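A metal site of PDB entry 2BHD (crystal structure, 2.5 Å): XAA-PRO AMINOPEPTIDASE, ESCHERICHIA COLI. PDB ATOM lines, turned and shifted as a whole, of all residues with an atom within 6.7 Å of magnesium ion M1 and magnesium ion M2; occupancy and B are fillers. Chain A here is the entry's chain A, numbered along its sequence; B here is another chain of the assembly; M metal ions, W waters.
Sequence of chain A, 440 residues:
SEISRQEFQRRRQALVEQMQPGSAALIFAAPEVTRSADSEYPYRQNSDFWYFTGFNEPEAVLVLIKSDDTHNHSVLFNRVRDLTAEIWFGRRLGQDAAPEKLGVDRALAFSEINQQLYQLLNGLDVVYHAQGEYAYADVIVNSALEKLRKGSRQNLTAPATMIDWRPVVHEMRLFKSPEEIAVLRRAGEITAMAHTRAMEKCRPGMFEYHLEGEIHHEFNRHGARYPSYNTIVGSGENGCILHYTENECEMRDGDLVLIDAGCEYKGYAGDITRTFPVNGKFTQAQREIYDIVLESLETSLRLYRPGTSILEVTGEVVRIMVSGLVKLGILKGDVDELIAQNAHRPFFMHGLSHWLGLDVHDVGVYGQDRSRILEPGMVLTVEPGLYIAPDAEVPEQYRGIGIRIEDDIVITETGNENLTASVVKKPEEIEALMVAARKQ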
ATOM      1  N   TYR A 229      23.870  29.974   7.015  1.00  0.00           N
ATOM      2  CA  TYR A 229      23.603  28.805   7.859  1.00  0.00           C
ATOM      3  C   TYR A 229      24.555  27.679   7.459  1.00  0.00           C
ATOM      4  O   TYR A 229      25.141  27.715   6.394  1.00  0.00           O
ATOM      5  CB  TYR A 229      22.135  28.321   7.726  1.00  0.00           C
ATOM      6  CG  TYR A 229      21.728  28.052   6.302  1.00  0.00           C
ATOM      7  CD1 TYR A 229      21.300  29.081   5.488  1.00  0.00           C
ATOM      8  CD2 TYR A 229      21.823  26.779   5.756  1.00  0.00           C
ATOM      9  CE1 TYR A 229      20.940  28.863   4.166  1.00  0.00           C
ATOM     10  CE2 TYR A 229      21.459  26.540   4.428  1.00  0.00           C
ATOM     11  CZ  TYR A 229      21.027  27.580   3.641  1.00  0.00           C
ATOM     12  OH  TYR A 229      20.658  27.381   2.328  1.00  0.00           O
ATOM     13  N   ILE A 232      24.489  22.136   3.929  1.00  0.00           N
ATOM     14  CA  ILE A 232      23.996  20.762   3.921  1.00  0.00           C
ATOM     15  C   ILE A 232      24.368  20.116   2.592  1.00  0.00           C
ATOM     16  O   ILE A 232      23.953  20.593   1.528  1.00  0.00           O
ATOM     17  CB  ILE A 232      22.452  20.742   4.103  1.00  0.00           C
ATOM     18  CG1 ILE A 232      22.067  21.222   5.521  1.00  0.00           C
ATOM     19  CG2 ILE A 232      21.858  19.356   3.813  1.00  0.00           C
ATOM     20  CD1 ILE A 232      20.680  21.814   5.596  1.00  0.00           C
ATOM     21  N   ASP A 260      21.767  22.097   0.351  1.00  0.00           N
ATOM     22  CA  ASP A 260      21.070  23.263   0.911  1.00  0.00           C
ATOM     23  C   ASP A 260      22.148  24.219   1.451  1.00  0.00           C
ATOM     24  O   ASP A 260      22.828  23.941   2.465  1.00  0.00           O
ATOM     25  CB  ASP A 260      20.068  22.854   2.010  1.00  0.00           C
ATOM     26  CG  ASP A 260      19.017  23.952   2.330  1.00  0.00           C
ATOM     27  OD1 ASP A 260      19.218  25.167   2.058  1.00  0.00           O
ATOM     28  OD2 ASP A 260      17.937  23.590   2.864  1.00  0.00           O
ATOM     29  N   ALA A 261      22.315  25.342   0.751  1.00  0.00           N
ATOM     30  CA  ALA A 261      23.352  26.307   1.075  1.00  0.00           C
ATOM     31  C   ALA A 261      22.951  27.708   0.690  1.00  0.00           C
ATOM     32  O   ALA A 261      22.216  27.923  -0.297  1.00  0.00           O
ATOM     33  CB  ALA A 261      24.635  25.935   0.415  1.00  0.00           C
ATOM     34  N   ASP A 271      19.183  31.376   0.311  1.00  0.00           N
ATOM     35  CA  ASP A 271      18.827  30.044   0.816  1.00  0.00           C
ATOM     36  C   ASP A 271      18.322  29.226  -0.365  1.00  0.00           C
ATOM     37  O   ASP A 271      17.170  29.357  -0.758  1.00  0.00           O
ATOM     38  CB  ASP A 271      17.764  30.143   1.923  1.00  0.00           C
ATOM     39  CG  ASP A 271      17.299  28.778   2.436  1.00  0.00           C
ATOM     40  OD1 ASP A 271      17.854  27.730   2.056  1.00  0.00           O
ATOM     41  OD2 ASP A 271      16.340  28.752   3.250  1.00  0.00           O
ATOM     42  N   ILE A 272      19.192  28.395  -0.924  1.00  0.00           N
ATOM     43  CA  ILE A 272      18.851  27.591  -2.083  1.00  0.00           C
ATOM     44  C   ILE A 272      19.082  26.103  -1.788  1.00  0.00           C
ATOM     45  O   ILE A 272      20.057  25.716  -1.127  1.00  0.00           O
ATOM     46  CB  ILE A 272      19.684  27.993  -3.321  1.00  0.00           C
ATOM     47  CG1 ILE A 272      19.294  29.386  -3.801  1.00  0.00           C
ATOM     48  CG2 ILE A 272      19.481  26.998  -4.475  1.00  0.00           C
ATOM     49  CD1 ILE A 272      20.074  29.824  -5.012  1.00  0.00           C
ATOM     50  N   THR A 273      18.185  25.271  -2.292  1.00  0.00           N
ATOM     51  CA  THR A 273      18.411  23.826  -2.289  1.00  0.00           C
ATOM     52  C   THR A 273      18.315  23.340  -3.714  1.00  0.00           C
ATOM     53  O   THR A 273      17.404  23.738  -4.444  1.00  0.00           O
ATOM     54  CB  THR A 273      17.418  23.042  -1.422  1.00  0.00           C
ATOM     55  OG1 THR A 273      17.309  23.635  -0.122  1.00  0.00           O
ATOM     56  CG2 THR A 273      17.884  21.588  -1.271  1.00  0.00           C
ATOM     57  N   HIS A 354       9.339  29.575   4.484  1.00  0.00           N
ATOM     58  CA  HIS A 354       9.579  30.431   5.634  1.00  0.00           C
ATOM     59  C   HIS A 354       9.981  31.813   5.155  1.00  0.00           C
ATOM     60  O   HIS A 354      10.482  31.941   4.059  1.00  0.00           O
ATOM     61  CB  HIS A 354      10.658  29.856   6.562  1.00  0.00           C
ATOM     62  CG  HIS A 354      11.963  29.533   5.880  1.00  0.00           C
ATOM     63  ND1 HIS A 354      12.928  30.478   5.636  1.00  0.00           N
ATOM     64  CD2 HIS A 354      12.457  28.353   5.427  1.00  0.00           C
ATOM     65  CE1 HIS A 354      13.965  29.904   5.042  1.00  0.00           C
ATOM     66  NE2 HIS A 354      13.699  28.618   4.901  1.00  0.00           N
ATOM     67  N   LEU A 356      12.287  35.058   4.725  1.00  0.00           N
ATOM     68  CA  LEU A 356      13.719  35.179   4.500  1.00  0.00           C
ATOM     69  C   LEU A 356      14.155  36.640   4.641  1.00  0.00           C
ATOM     70  O   LEU A 356      13.468  37.553   4.157  1.00  0.00           O
ATOM     71  CB  LEU A 356      14.050  34.687   3.094  1.00  0.00           C
ATOM     72  CG  LEU A 356      15.513  34.586   2.684  1.00  0.00           C
ATOM     73  CD1 LEU A 356      16.215  33.495   3.475  1.00  0.00           C
ATOM     74  CD2 LEU A 356      15.589  34.321   1.178  1.00  0.00           C
ATOM     75  N   VAL A 360      17.957  33.638   8.038  1.00  0.00           N
ATOM     76  CA  VAL A 360      17.506  32.707   7.032  1.00  0.00           C
ATOM     77  C   VAL A 360      16.072  32.235   7.355  1.00  0.00           C
ATOM     78  O   VAL A 360      15.238  32.185   6.468  1.00  0.00           O
ATOM     79  CB  VAL A 360      18.494  31.532   6.791  1.00  0.00           C
ATOM     80  CG1 VAL A 360      18.667  30.673   8.033  1.00  0.00           C
ATOM     81  CG2 VAL A 360      18.015  30.669   5.619  1.00  0.00           C
ATOM     82  N   HIS A 361      15.799  31.917   8.605  1.00  0.00           N
ATOM     83  CA  HIS A 361      14.434  31.699   9.084  1.00  0.00           C
ATOM     84  C   HIS A 361      13.988  33.011   9.690  1.00  0.00           C
ATOM     85  O   HIS A 361      14.132  33.229  10.898  1.00  0.00           O
ATOM     86  CB  HIS A 361      14.353  30.612  10.155  1.00  0.00           C
ATOM     87  CG  HIS A 361      14.670  29.244   9.655  1.00  0.00           C
ATOM     88  ND1 HIS A 361      15.031  28.211  10.498  1.00  0.00           N
ATOM     89  CD2 HIS A 361      14.699  28.729   8.404  1.00  0.00           C
ATOM     90  CE1 HIS A 361      15.258  27.127   9.782  1.00  0.00           C
ATOM     91  NE2 HIS A 361      15.061  27.407   8.510  1.00  0.00           N
ATOM     92  N   THR A 381      10.857  31.597   1.134  1.00  0.00           N
ATOM     93  CA  THR A 381      11.363  30.444   0.414  1.00  0.00           C
ATOM     94  C   THR A 381      10.208  29.581  -0.115  1.00  0.00           C
ATOM     95  O   THR A 381       9.079  29.636   0.391  1.00  0.00           O
ATOM     96  CB  THR A 381      12.282  29.583   1.277  1.00  0.00           C
ATOM     97  OG1 THR A 381      11.547  29.039   2.384  1.00  0.00           O
ATOM     98  CG2 THR A 381      13.454  30.423   1.793  1.00  0.00           C
ATOM     99  N   VAL A 382      10.502  28.818  -1.166  1.00  0.00           N
ATOM    100  CA  VAL A 382       9.575  27.834  -1.682  1.00  0.00           C
ATOM    101  C   VAL A 382      10.384  26.550  -1.800  1.00  0.00           C
ATOM    102  O   VAL A 382      11.261  26.456  -2.665  1.00  0.00           O
ATOM    103  CB  VAL A 382       8.987  28.242  -3.039  1.00  0.00           C
ATOM    104  CG1 VAL A 382       7.858  27.291  -3.430  1.00  0.00           C
ATOM    105  CG2 VAL A 382       8.471  29.670  -2.998  1.00  0.00           C
ATOM    106  N   GLU A 383      10.107  25.587  -0.937  1.00  0.00           N
ATOM    107  CA  GLU A 383      10.980  24.444  -0.784  1.00  0.00           C
ATOM    108  C   GLU A 383      10.268  23.121  -0.524  1.00  0.00           C
ATOM    109  O   GLU A 383      10.442  22.523   0.534  1.00  0.00           O
ATOM    110  CB  GLU A 383      11.997  24.718   0.315  1.00  0.00           C
ATOM    111  CG  GLU A 383      11.434  25.076   1.675  1.00  0.00           C
ATOM    112  CD  GLU A 383      12.536  25.337   2.679  1.00  0.00           C
ATOM    113  OE1 GLU A 383      13.403  24.447   2.846  1.00  0.00           O
ATOM    114  OE2 GLU A 383      12.575  26.442   3.271  1.00  0.00           O
ATOM    115  N   ARG A 404      14.921  17.807  -2.352  1.00  0.00           N
ATOM    116  CA  ARG A 404      14.336  19.105  -2.074  1.00  0.00           C
ATOM    117  C   ARG A 404      14.821  20.067  -3.139  1.00  0.00           C
ATOM    118  O   ARG A 404      15.965  19.979  -3.574  1.00  0.00           O
ATOM    119  CB  ARG A 404      14.723  19.605  -0.684  1.00  0.00           C
ATOM    120  CG  ARG A 404      14.242  21.003  -0.335  1.00  0.00           C
ATOM    121  CD  ARG A 404      14.268  21.306   1.167  1.00  0.00           C
ATOM    122  NE  ARG A 404      15.610  21.409   1.751  1.00  0.00           N
ATOM    123  CZ  ARG A 404      16.203  20.491   2.513  1.00  0.00           C
ATOM    124  NH1 ARG A 404      15.621  19.321   2.777  1.00  0.00           N
ATOM    125  NH2 ARG A 404      17.407  20.709   3.012  1.00  0.00           N
ATOM    126  N   GLU A 406      14.614  24.302  -3.703  1.00  0.00           N
ATOM    127  CA  GLU A 406      14.258  25.519  -2.981  1.00  0.00           C
ATOM    128  C   GLU A 406      14.692  26.767  -3.757  1.00  0.00           C
ATOM    129  O   GLU A 406      15.835  26.890  -4.162  1.00  0.00           O
ATOM    130  CB  GLU A 406      14.884  25.503  -1.575  1.00  0.00           C
ATOM    131  CG  GLU A 406      14.844  26.827  -0.786  1.00  0.00           C
ATOM    132  CD  GLU A 406      15.265  26.654   0.679  1.00  0.00           C
ATOM    133  OE1 GLU A 406      16.169  25.809   0.960  1.00  0.00           O
ATOM    134  OE2 GLU A 406      14.713  27.356   1.563  1.00  0.00           O
ATOM    135  N   ASP A 408      14.107  31.244  -3.668  1.00  0.00           N
ATOM    136  CA  ASP A 408      13.784  32.410  -2.841  1.00  0.00           C
ATOM    137  C   ASP A 408      13.008  33.413  -3.686  1.00  0.00           C
ATOM    138  O   ASP A 408      13.397  33.717  -4.820  1.00  0.00           O
ATOM    139  CB  ASP A 408      15.068  33.093  -2.335  1.00  0.00           C
ATOM    140  CG  ASP A 408      15.997  32.129  -1.598  1.00  0.00           C
ATOM    141  OD1 ASP A 408      15.490  31.148  -1.004  1.00  0.00           O
ATOM    142  OD2 ASP A 408      17.219  32.368  -1.623  1.00  0.00           O
ATOM    143  N   PRO B   2      14.900  23.946   6.026  1.00  0.00           N
ATOM    144  CA  PRO B   2      13.455  23.817   6.187  1.00  0.00           C
ATOM    145  C   PRO B   2      12.982  24.257   7.560  1.00  0.00           C
ATOM    146  O   PRO B   2      13.748  24.158   8.535  1.00  0.00           O
ATOM    147  CB  PRO B   2      13.236  22.314   6.012  1.00  0.00           C
ATOM    148  CG  PRO B   2      14.298  21.874   5.117  1.00  0.00           C
ATOM    149  CD  PRO B   2      15.485  22.763   5.372  1.00  0.00           C
ATOM    150  N   LEU B   3      11.752  24.758   7.626  1.00  0.00           N
ATOM    151  CA  LEU B   3      11.058  25.102   8.876  1.00  0.00           C
ATOM    152  C   LEU B   3       9.731  24.328   8.909  1.00  0.00           C
ATOM    153  O   LEU B   3       9.338  23.754   9.930  1.00  0.00           O
ATOM    154  CB  LEU B   3      10.809  26.624   8.982  1.00  0.00           C
ATOM    155  CG  LEU B   3      10.386  27.255  10.331  1.00  0.00           C
ATOM    156  CD1 LEU B   3      11.394  27.021  11.442  1.00  0.00           C
ATOM    157  CD2 LEU B   3      10.149  28.740  10.180  1.00  0.00           C
ATOM    158  OXT LEU B   3       9.017  24.228   7.916  1.00  0.00           O
HETATM  159 MG    MG M   1      14.763  27.405   3.517  1.00  0.00          MG
HETATM  160 MG    MG M   2      17.176  25.985   2.751  1.00  0.00          MG
HETATM  161  O   HOH W   1      15.724  25.690   3.897  1.00  0.00           O
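The backbone NH (N) of Asp 271 is in hydrogen-bond range of the side-chain carboxylate (OD2) of Asp 408.
The backbone carbonyl oxygen (O) of His 354 sits at hydrogen-bond distance from the backbone NH (N) of Thr 381 (3.0 Å).
OG1 of Thr 273 lies close to OD2 of Asp 260, 3.1 Å away.
ND1 of His 354 sits close to O of Val 360.
OH of Tyr 229 lies close to N of Ala 261, at 3.1 Å.
The side-chain carboxylate (OE2) of Glu 383 lies close to the side-chain hydroxyl (OG1) of Thr 381 (2.9 Å).
OD1 of Asp 271 sits close to OH of Tyr 229.
The side-chain hydroxyl (OG1) of Thr 273 lies within hydrogen-bond range of the guanidinium group (NE) of Arg 404 (3.4 Å).
Residues that only touch magnesium ion M1: Thr 381.
Five residues have an atom within 4 Å of magnesium ion M1: Asp 271, His 354, Thr 381, Glu 383 and Glu 406.
The nearest printed residue that does not touch magnesium ion M1 is Pro 2 of chain B (4.3 Å).
Residues that only touch magnesium ion M2: Thr 273 and Tyr 229.
Within 4 Å of magnesium ion M2: Tyr 229, Asp 260, Asp 271, Thr 273 and Glu 406.
Magnesium ion M1 is bound by OE2 of Glu 406.
Magnesium ion M1 is bound by water W1 (2.0 Å).
The side-chain carboxylate (OD2) of Asp 271 is bound to magnesium ion M1, at 2.1 Å.
Magnesium ion M1 is bound by NE2 of His 354 (2.1 Å).
OE2 of Glu 383 binds magnesium ion M1 (2.4 Å).
Magnesium ion M2 is bound by water W1, the side-chain carboxylate (OD1) of Asp 271, the side-chain carboxylate (OE1) of Glu 406, the side-chain carboxylate (OD1) of Asp 260 and the side-chain carboxylate (OD2) of Asp 260.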
